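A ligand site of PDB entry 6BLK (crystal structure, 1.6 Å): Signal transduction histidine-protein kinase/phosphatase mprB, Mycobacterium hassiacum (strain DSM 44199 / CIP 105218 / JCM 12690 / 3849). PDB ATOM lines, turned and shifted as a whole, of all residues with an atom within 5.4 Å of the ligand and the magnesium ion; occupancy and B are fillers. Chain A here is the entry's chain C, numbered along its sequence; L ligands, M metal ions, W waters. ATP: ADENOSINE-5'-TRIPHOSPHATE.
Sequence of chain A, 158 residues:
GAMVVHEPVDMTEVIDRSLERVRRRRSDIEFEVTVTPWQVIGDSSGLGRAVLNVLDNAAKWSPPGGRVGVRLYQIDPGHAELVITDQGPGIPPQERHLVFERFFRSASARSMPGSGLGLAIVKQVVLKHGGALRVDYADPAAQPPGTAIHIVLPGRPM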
ATOM      1  N   ASN A  53     -14.174 -29.514  11.976  1.00  0.00           N
ATOM      2  CA  ASN A  53     -14.485 -28.354  11.162  1.00  0.00           C
ATOM      3  C   ASN A  53     -14.567 -27.081  11.999  1.00  0.00           C
ATOM      4  O   ASN A  53     -14.161 -26.004  11.545  1.00  0.00           O
ATOM      5  CB  ASN A  53     -15.802 -28.568  10.400  1.00  0.00           C
ATOM      6  CG  ASN A  53     -15.661 -29.544   9.234  1.00  0.00           C
ATOM      7  OD1 ASN A  53     -14.613 -30.132   8.993  1.00  0.00           O
ATOM      8  ND2 ASN A  53     -16.745 -29.716   8.514  1.00  0.00           N
ATOM      9  N   ASP A  56     -11.003 -26.213  13.084  1.00  0.00           N
ATOM     10  CA  ASP A  56     -10.243 -25.688  11.962  1.00  0.00           C
ATOM     11  C   ASP A  56     -10.527 -24.203  11.750  1.00  0.00           C
ATOM     12  O   ASP A  56      -9.598 -23.424  11.510  1.00  0.00           O
ATOM     13  CB  ASP A  56     -10.543 -26.475  10.691  1.00  0.00           C
ATOM     14  CG  ASP A  56      -9.643 -26.074   9.551  1.00  0.00           C
ATOM     15  OD1 ASP A  56      -8.425 -26.274   9.688  1.00  0.00           O
ATOM     16  OD2 ASP A  56     -10.185 -25.547   8.546  1.00  0.00           O
ATOM     17  N   ASN A  57     -11.798 -23.784  11.852  1.00  0.00           N
ATOM     18  CA  ASN A  57     -12.140 -22.371  11.726  1.00  0.00           C
ATOM     19  C   ASN A  57     -11.529 -21.580  12.856  1.00  0.00           C
ATOM     20  O   ASN A  57     -10.990 -20.476  12.647  1.00  0.00           O
ATOM     21  CB  ASN A  57     -13.666 -22.147  11.725  1.00  0.00           C
ATOM     22  CG  ASN A  57     -14.329 -22.724  10.503  1.00  0.00           C
ATOM     23  OD1 ASN A  57     -13.695 -22.927   9.460  1.00  0.00           O
ATOM     24  ND2 ASN A  57     -15.631 -22.997  10.627  1.00  0.00           N
ATOM     25  N   ALA A  58     -11.577 -22.121  14.072  1.00  0.00           N
ATOM     26  CA  ALA A  58     -11.049 -21.411  15.202  1.00  0.00           C
ATOM     27  C   ALA A  58      -9.571 -21.157  14.988  1.00  0.00           C
ATOM     28  O   ALA A  58      -9.064 -20.060  15.284  1.00  0.00           O
ATOM     29  CB  ALA A  58     -11.282 -22.205  16.498  1.00  0.00           C
ATOM     30  N   LYS A  60      -7.953 -21.101  11.988  1.00  0.00           N
ATOM     31  CA  LYS A  60      -7.677 -20.299  10.792  1.00  0.00           C
ATOM     32  C   LYS A  60      -7.657 -18.831  11.130  1.00  0.00           C
ATOM     33  O   LYS A  60      -6.754 -18.078  10.691  1.00  0.00           O
ATOM     34  CB  LYS A  60      -8.709 -20.572   9.689  1.00  0.00           C
ATOM     35  CG  LYS A  60      -8.446 -21.836   8.902  1.00  0.00           C
ATOM     36  CD  LYS A  60      -9.655 -22.210   8.033  1.00  0.00           C
ATOM     37  CE  LYS A  60      -9.878 -21.231   6.908  1.00  0.00           C
ATOM     38  NZ  LYS A  60     -11.066 -21.555   6.019  1.00  0.00           N
ATOM     39  N   TRP A  61      -8.645 -18.391  11.908  1.00  0.00           N
ATOM     40  CA  TRP A  61      -8.830 -16.980  12.208  1.00  0.00           C
ATOM     41  C   TRP A  61      -8.306 -16.607  13.595  1.00  0.00           C
ATOM     42  O   TRP A  61      -8.581 -15.506  14.080  1.00  0.00           O
ATOM     43  CB  TRP A  61     -10.300 -16.613  12.013  1.00  0.00           C
ATOM     44  CG  TRP A  61     -10.641 -16.547  10.537  1.00  0.00           C
ATOM     45  CD1 TRP A  61     -10.304 -15.562   9.669  1.00  0.00           C
ATOM     46  CD2 TRP A  61     -11.356 -17.531   9.761  1.00  0.00           C
ATOM     47  NE1 TRP A  61     -10.763 -15.860   8.401  1.00  0.00           N
ATOM     48  CE2 TRP A  61     -11.426 -17.058   8.436  1.00  0.00           C
ATOM     49  CE3 TRP A  61     -11.956 -18.761  10.076  1.00  0.00           C
ATOM     50  CZ2 TRP A  61     -12.032 -17.780   7.423  1.00  0.00           C
ATOM     51  CZ3 TRP A  61     -12.572 -19.473   9.060  1.00  0.00           C
ATOM     52  CH2 TRP A  61     -12.613 -18.981   7.748  1.00  0.00           C
ATOM     53  N   ASP A  86     -12.428 -18.688  20.098  1.00  0.00           N
ATOM     54  CA  ASP A  86     -11.144 -18.139  19.636  1.00  0.00           C
ATOM     55  C   ASP A  86     -11.066 -16.659  19.981  1.00  0.00           C
ATOM     56  O   ASP A  86     -11.977 -16.067  20.566  1.00  0.00           O
ATOM     57  CB  ASP A  86     -10.944 -18.371  18.132  1.00  0.00           C
ATOM     58  CG  ASP A  86     -12.027 -17.727  17.316  1.00  0.00           C
ATOM     59  OD1 ASP A  86     -12.206 -16.482  17.399  1.00  0.00           O
ATOM     60  OD2 ASP A  86     -12.746 -18.478  16.618  1.00  0.00           O
ATOM     61  N   PRO A  89     -11.680 -12.225  14.985  1.00  0.00           N
ATOM     62  CA  PRO A  89     -12.519 -11.022  14.886  1.00  0.00           C
ATOM     63  C   PRO A  89     -13.941 -11.203  15.371  1.00  0.00           C
ATOM     64  O   PRO A  89     -14.618 -10.203  15.654  1.00  0.00           O
ATOM     65  CB  PRO A  89     -12.503 -10.709  13.395  1.00  0.00           C
ATOM     66  CG  PRO A  89     -12.279 -12.034  12.770  1.00  0.00           C
ATOM     67  CD  PRO A  89     -11.306 -12.725  13.651  1.00  0.00           C
ATOM     68  N   GLY A  90     -14.423 -12.437  15.466  1.00  0.00           N
ATOM     69  CA  GLY A  90     -15.807 -12.665  15.814  1.00  0.00           C
ATOM     70  C   GLY A  90     -16.706 -12.490  14.607  1.00  0.00           C
ATOM     71  O   GLY A  90     -16.382 -11.839  13.624  1.00  0.00           O
ATOM     72  N   ILE A  91     -17.888 -13.094  14.695  1.00  0.00           N
ATOM     73  CA  ILE A  91     -18.916 -12.957  13.664  1.00  0.00           C
ATOM     74  C   ILE A  91     -19.987 -12.018  14.207  1.00  0.00           C
ATOM     75  O   ILE A  91     -20.586 -12.313  15.245  1.00  0.00           O
ATOM     76  CB  ILE A  91     -19.512 -14.320  13.287  1.00  0.00           C
ATOM     77  CG1 ILE A  91     -18.433 -15.179  12.607  1.00  0.00           C
ATOM     78  CG2 ILE A  91     -20.740 -14.139  12.369  1.00  0.00           C
ATOM     79  CD1 ILE A  91     -18.820 -16.640  12.386  1.00  0.00           C
ATOM     80  N   PHE A 104     -21.489 -19.109   2.928  1.00  0.00           N
ATOM     81  CA  PHE A 104     -21.323 -17.899   3.740  1.00  0.00           C
ATOM     82  C   PHE A 104     -19.853 -17.530   3.885  1.00  0.00           C
ATOM     83  O   PHE A 104     -18.989 -18.404   4.016  1.00  0.00           O
ATOM     84  CB  PHE A 104     -21.929 -18.102   5.130  1.00  0.00           C
ATOM     85  CG  PHE A 104     -21.558 -17.002   6.095  1.00  0.00           C
ATOM     86  CD1 PHE A 104     -21.966 -15.705   5.873  1.00  0.00           C
ATOM     87  CD2 PHE A 104     -20.779 -17.271   7.211  1.00  0.00           C
ATOM     88  CE1 PHE A 104     -21.625 -14.700   6.740  1.00  0.00           C
ATOM     89  CE2 PHE A 104     -20.446 -16.272   8.080  1.00  0.00           C
ATOM     90  CZ  PHE A 104     -20.868 -14.983   7.840  1.00  0.00           C
ATOM     91  N   ARG A 105     -19.572 -16.224   3.779  1.00  0.00           N
ATOM     92  CA  ARG A 105     -18.243 -15.672   3.987  1.00  0.00           C
ATOM     93  C   ARG A 105     -18.401 -14.356   4.738  1.00  0.00           C
ATOM     94  O   ARG A 105     -19.065 -13.446   4.228  1.00  0.00           O
ATOM     95  CB  ARG A 105     -17.562 -15.456   2.615  1.00  0.00           C
ATOM     96  CG  ARG A 105     -16.064 -15.544   2.605  1.00  0.00           C
ATOM     97  CD  ARG A 105     -15.564 -15.618   1.175  1.00  0.00           C
ATOM     98  NE  ARG A 105     -14.106 -15.637   1.127  1.00  0.00           N
ATOM     99  CZ  ARG A 105     -13.348 -16.716   1.011  1.00  0.00           C
ATOM    100  NH1 ARG A 105     -13.871 -17.941   0.939  1.00  0.00           N
ATOM    101  NH2 ARG A 105     -12.036 -16.592   0.965  1.00  0.00           N
ATOM    102  N   SER A 106     -17.796 -14.255   5.925  1.00  0.00           N
ATOM    103  CA  SER A 106     -17.870 -13.044   6.725  1.00  0.00           C
ATOM    104  C   SER A 106     -16.957 -11.937   6.189  1.00  0.00           C
ATOM    105  O   SER A 106     -15.775 -12.169   5.946  1.00  0.00           O
ATOM    106  CB  SER A 106     -17.504 -13.366   8.173  1.00  0.00           C
ATOM    107  OG  SER A 106     -17.594 -12.213   8.988  1.00  0.00           O
ATOM    108  N   ALA A 109     -13.886 -11.277   8.642  1.00  0.00           N
ATOM    109  CA  ALA A 109     -12.805 -12.233   8.734  1.00  0.00           C
ATOM    110  C   ALA A 109     -11.989 -12.172   7.449  1.00  0.00           C
ATOM    111  O   ALA A 109     -12.555 -12.017   6.359  1.00  0.00           O
ATOM    112  CB  ALA A 109     -13.339 -13.645   8.961  1.00  0.00           C
ATOM    113  N   MET A 112      -9.637 -16.368   3.175  1.00  0.00           N
ATOM    114  CA  MET A 112      -8.772 -17.525   3.224  1.00  0.00           C
ATOM    115  C   MET A 112      -9.309 -18.613   2.328  1.00  0.00           C
ATOM    116  O   MET A 112     -10.525 -18.677   2.079  1.00  0.00           O
ATOM    117  CB  MET A 112      -8.604 -18.069   4.636  1.00  0.00           C
ATOM    118  CG  MET A 112      -7.974 -17.071   5.603  1.00  0.00           C
ATOM    119  SD  MET A 112      -7.808 -17.756   7.251  1.00  0.00           S
ATOM    120  CE  MET A 112      -6.435 -18.899   7.004  1.00  0.00           C
ATOM    121  N   PRO A 113      -8.457 -19.478   1.799  1.00  0.00           N
ATOM    122  CA  PRO A 113      -8.939 -20.576   0.963  1.00  0.00           C
ATOM    123  C   PRO A 113      -9.950 -21.411   1.722  1.00  0.00           C
ATOM    124  O   PRO A 113      -9.801 -21.654   2.916  1.00  0.00           O
ATOM    125  CB  PRO A 113      -7.667 -21.377   0.648  1.00  0.00           C
ATOM    126  CG  PRO A 113      -6.570 -20.353   0.727  1.00  0.00           C
ATOM    127  CD  PRO A 113      -6.978 -19.394   1.808  1.00  0.00           C
ATOM    128  N   GLY A 114     -10.959 -21.872   1.007  1.00  0.00           N
ATOM    129  CA  GLY A 114     -12.054 -22.616   1.580  1.00  0.00           C
ATOM    130  C   GLY A 114     -13.320 -22.140   0.918  1.00  0.00           C
ATOM    131  O   GLY A 114     -13.491 -20.934   0.727  1.00  0.00           O
ATOM    132  N   SER A 115     -14.234 -23.045   0.582  1.00  0.00           N
ATOM    133  CA  SER A 115     -15.394 -22.630  -0.202  1.00  0.00           C
ATOM    134  C   SER A 115     -16.679 -22.544   0.604  1.00  0.00           C
ATOM    135  O   SER A 115     -17.754 -22.391   0.011  1.00  0.00           O
ATOM    136  CB  SER A 115     -15.559 -23.546  -1.404  1.00  0.00           C
ATOM    137  OG  SER A 115     -14.636 -23.160  -2.404  1.00  0.00           O
ATOM    138  N   GLY A 116     -16.603 -22.610   1.926  1.00  0.00           N
ATOM    139  CA  GLY A 116     -17.765 -22.316   2.749  1.00  0.00           C
ATOM    140  C   GLY A 116     -18.711 -23.466   2.925  1.00  0.00           C
ATOM    141  O   GLY A 116     -19.924 -23.283   2.878  1.00  0.00           O
ATOM    142  N   LEU A 117     -18.182 -24.675   3.127  1.00  0.00           N
ATOM    143  CA  LEU A 117     -18.997 -25.845   3.338  1.00  0.00           C
ATOM    144  C   LEU A 117     -18.865 -26.435   4.732  1.00  0.00           C
ATOM    145  O   LEU A 117     -19.747 -27.201   5.130  1.00  0.00           O
ATOM    146  CB  LEU A 117     -18.615 -26.916   2.310  1.00  0.00           C
ATOM    147  CG  LEU A 117     -18.796 -26.466   0.851  1.00  0.00           C
ATOM    148  CD1 LEU A 117     -18.044 -27.379  -0.085  1.00  0.00           C
ATOM    149  CD2 LEU A 117     -20.260 -26.441   0.466  1.00  0.00           C
ATOM    150  N   GLY A 118     -17.827 -26.057   5.500  1.00  0.00           N
ATOM    151  CA  GLY A 118     -17.515 -26.747   6.751  1.00  0.00           C
ATOM    152  C   GLY A 118     -18.628 -26.626   7.779  1.00  0.00           C
ATOM    153  O   GLY A 118     -18.953 -27.607   8.471  1.00  0.00           O
ATOM    154  N   LEU A 119     -19.186 -25.446   7.939  1.00  0.00           N
ATOM    155  CA  LEU A 119     -20.171 -25.254   8.999  1.00  0.00           C
ATOM    156  C   LEU A 119     -21.544 -25.786   8.605  1.00  0.00           C
ATOM    157  O   LEU A 119     -22.297 -26.225   9.460  1.00  0.00           O
ATOM    158  CB  LEU A 119     -20.268 -23.798   9.382  1.00  0.00           C
ATOM    159  CG  LEU A 119     -19.094 -23.310  10.249  1.00  0.00           C
ATOM    160  CD1 LEU A 119     -19.206 -21.815  10.459  1.00  0.00           C
ATOM    161  CD2 LEU A 119     -19.001 -23.983  11.579  1.00  0.00           C
ATOM    162  N   ALA A 120     -21.884 -25.766   7.321  1.00  0.00           N
ATOM    163  CA  ALA A 120     -23.082 -26.496   6.889  1.00  0.00           C
ATOM    164  C   ALA A 120     -23.012 -27.985   7.255  1.00  0.00           C
ATOM    165  O   ALA A 120     -24.026 -28.580   7.645  1.00  0.00           O
ATOM    166  CB  ALA A 120     -23.275 -26.330   5.379  1.00  0.00           C
ATOM    167  N   THR A 147     -14.963 -15.544  18.220  1.00  0.00           N
ATOM    168  CA  THR A 147     -16.174 -16.329  17.961  1.00  0.00           C
ATOM    169  C   THR A 147     -16.307 -17.456  18.950  1.00  0.00           C
ATOM    170  O   THR A 147     -15.336 -18.115  19.318  1.00  0.00           O
ATOM    171  CB  THR A 147     -16.162 -16.909  16.542  1.00  0.00           C
ATOM    172  OG1 THR A 147     -16.005 -15.863  15.597  1.00  0.00           O
ATOM    173  CG2 THR A 147     -17.484 -17.621  16.204  1.00  0.00           C
HETATM  174  PG  ATP L   1     -14.398 -24.717   4.508  1.00  0.00           P
HETATM  175  O1G ATP L   1     -14.750 -24.817   5.983  1.00  0.00           O
HETATM  176  O2G ATP L   1     -15.428 -25.258   3.498  1.00  0.00           O
HETATM  177  O3G ATP L   1     -12.974 -25.119   4.182  1.00  0.00           O
HETATM  178  PB  ATP L   1     -14.702 -21.898   5.249  1.00  0.00           P
HETATM  179  O1B ATP L   1     -14.553 -20.608   4.463  1.00  0.00           O
HETATM  180  O2B ATP L   1     -13.811 -22.211   6.403  1.00  0.00           O
HETATM  181  O3B ATP L   1     -14.439 -23.119   4.196  1.00  0.00           O
HETATM  182  PA  ATP L   1     -16.987 -22.351   7.028  1.00  0.00           P
HETATM  183  O1A ATP L   1     -18.373 -22.905   6.696  1.00  0.00           O
HETATM  184  O2A ATP L   1     -16.108 -23.163   7.938  1.00  0.00           O
HETATM  185  O3A ATP L   1     -16.297 -22.065   5.576  1.00  0.00           O
HETATM  186  O5' ATP L   1     -17.182 -20.891   7.546  1.00  0.00           O
HETATM  187  C5' ATP L   1     -17.948 -19.959   6.801  1.00  0.00           C
HETATM  188  C4' ATP L   1     -17.340 -18.567   6.985  1.00  0.00           C
HETATM  189  O4' ATP L   1     -17.669 -18.145   8.315  1.00  0.00           O
HETATM  190  C3' ATP L   1     -15.819 -18.434   6.851  1.00  0.00           C
HETATM  191  O3' ATP L   1     -15.395 -18.237   5.485  1.00  0.00           O
HETATM  192  C2' ATP L   1     -15.571 -17.203   7.716  1.00  0.00           C
HETATM  193  O2' ATP L   1     -15.895 -15.990   7.011  1.00  0.00           O
HETATM  194  C1' ATP L   1     -16.599 -17.353   8.810  1.00  0.00           C
HETATM  195  N9  ATP L   1     -16.087 -18.038  10.012  1.00  0.00           N
HETATM  196  C8  ATP L   1     -16.334 -19.323  10.433  1.00  0.00           C
HETATM  197  N7  ATP L   1     -15.709 -19.561  11.618  1.00  0.00           N
HETATM  198  C5  ATP L   1     -15.073 -18.424  11.957  1.00  0.00           C
HETATM  199  C6  ATP L   1     -14.278 -18.027  13.100  1.00  0.00           C
HETATM  200  N6  ATP L   1     -14.018 -18.929  14.056  1.00  0.00           N
HETATM  201  N1  ATP L   1     -13.806 -16.778  13.113  1.00  0.00           N
HETATM  202  C2  ATP L   1     -14.059 -15.896  12.134  1.00  0.00           C
HETATM  203  N3  ATP L   1     -14.804 -16.192  11.055  1.00  0.00           N
HETATM  204  C4  ATP L   1     -15.336 -17.429  10.935  1.00  0.00           C
HETATM  205 MG    MG M   1     -14.280 -23.838   7.653  1.00  0.00          MG
HETATM  206  O   HOH W   1     -10.613 -23.794   4.524  1.00  0.00           O
HETATM  207  O   HOH W   2     -16.597 -21.763  13.141  1.00  0.00           O
HETATM  208  O   HOH W   3     -14.617 -25.604   8.763  1.00  0.00           O
HETATM  209  O   HOH W   4     -13.752 -14.757   5.420  1.00  0.00           O
HETATM  210  O   HOH W   5     -11.828 -27.265   5.317  1.00  0.00           O
HETATM  211  O   HOH W   6     -14.783 -21.769  15.098  1.00  0.00           O
HETATM  212  O   HOH W   7     -13.901 -27.493   7.319  1.00  0.00           O
HETATM  213  O   HOH W   8     -20.783 -23.817   5.497  1.00  0.00           O
HETATM  214  O   HOH W   9     -21.426 -21.271   6.930  1.00  0.00           O
HETATM  215  O   HOH W  10     -12.196 -19.447   4.314  1.00  0.00           O
HETATM  216  O   HOH W  11     -13.307 -15.212  15.325  1.00  0.00           O
HETATM  217  O   HOH W  12     -16.416 -19.248   2.704  1.00  0.00           O
HETATM  218  O   HOH W  13     -12.457 -25.936   1.728  1.00  0.00           O
HETATM  219  O   HOH W  14     -15.366 -28.027   3.628  1.00  0.00           O
HETATM  220  O   HOH W  15     -12.107 -24.326   7.375  1.00  0.00           O
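Water W15 lies within hydrogen-bond range of the side-chain carboxylate (OD2) of Asp 56 (2.6 Å), the side-chain amino group (NZ) of Lys 60 (3.3 Å) and an oxygen (O3G) of the ligand (3.4 Å). Water W10 lies within hydrogen-bond range of O1B of the ligand (2.6 Å), O of Met 112 (2.9 Å) and NZ of Lys 60 (2.9 Å). Water W11 lies within hydrogen-bond range of OD1 of Asp 86 (2.7 Å), N1 of the ligand (2.8 Å), OG1 of Thr 147 (2.8 Å) and N of Gly 90 (3.0 Å). Water W8 lies within hydrogen-bond range of the backbone carbonyl oxygen of Gly 116, an oxygen (O1A) of the ligand, the backbone NH of Ala 120 and the backbone NH of Leu 119. Water W12 lies within hydrogen-bond range of an oxygen (O1B) of the ligand (2.9 Å), the backbone carbonyl oxygen of Phe 104 (3.0 Å), the guanidinium group of Arg 105 (3.4 Å) and the backbone NH of Gly 116 (3.5 Å). Water W6 lies within hydrogen-bond range of N6 of the ligand (3.1 Å) and N of Ala 58 (3.4 Å).
The backbone NH of Ser 106 sits at hydrogen-bond distance from an oxygen (O2') of the ligand. The backbone NH (N) of Leu 117 lies within hydrogen-bond range of an oxygen (O2G) of the ligand (2.8 Å). O1B of the ligand is in salt-bridge range of NZ of Lys 60 (3.9 Å). The side-chain carboxylate (OD2) of Asp 86 is in hydrogen-bond range of a nitrogen (N6) of the ligand (2.9 Å). An oxygen (O1A) of the ligand is in hydrogen-bond range of the backbone NH (N) of Leu 119. An oxygen (O3B) of the ligand lies within hydrogen-bond range of the backbone NH of Gly 116, at 3.2 Å. The backbone NH (N) of Gly 118 is in hydrogen-bond range of an oxygen (O2G) of the ligand, 3.2 Å away. The side-chain hydroxyl (OG1) of Thr 147 is in hydrogen-bond range of a nitrogen (N1) of the ligand, at 3.4 Å.
One residue has an atom within 4 Å of the magnesium ion: Asn 57. The nearest printed residue that does not touch the magnesium ion is Lys 60 (4.3 Å).
Trp 61 touches the ligand. Ile 91 touches the ligand (CD1 to C4, 3.9 Å). Phe 104 touches the ligand. Arg 105 touches the ligand (C to O2', 3.8 Å). CB of Ala 109 touches N3 of the ligand, 3.6 Å away. Gly 114 touches the ligand (CA to O3B, 3.6 Å). N of Ser 115 touches O3B of the ligand (3.6 Å). The nearest printed residue that does not touch the ligand is Ala 58 (4.02 Å).
The magnesium ion is bound by O2A of the ligand (2.0 Å), O1G of the ligand (2.0 Å), O2B of the ligand (2.1 Å), OD1 of Asn 57 (2.1 Å), water W3 (2.1 Å) and water W15 (2.2 Å).
The side-chain amide nitrogen (ND2) of Asn 57 sits close to the backbone carbonyl oxygen (O) of Asn 53 (3.5 Å). NZ of Lys 60 lies within hydrogen-bond range of O of Pro 113, at 3.4 Å. The backbone NH (N) of Thr 147 sits at hydrogen-bond distance from the side-chain carboxylate (OD1) of Asp 86 (3.0 Å). The backbone carbonyl oxygen (O) of Gly 118 lies within hydrogen-bond range of the side-chain amide nitrogen (ND2) of Asn 53 (3.1 Å). NE1 of Trp 61 sits at hydrogen-bond distance from SD of Met 112. The side-chain hydroxyl of Thr 147 is in hydrogen-bond range of the backbone NH of Ile 91. The guanidinium group (NH1) of Arg 105 sits at hydrogen-bond distance from the backbone carbonyl oxygen (O) of Gly 114 (3.0 Å). The backbone carbonyl oxygen of Met 112 is in hydrogen-bond range of the guanidinium group of Arg 105 (2.8 Å).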
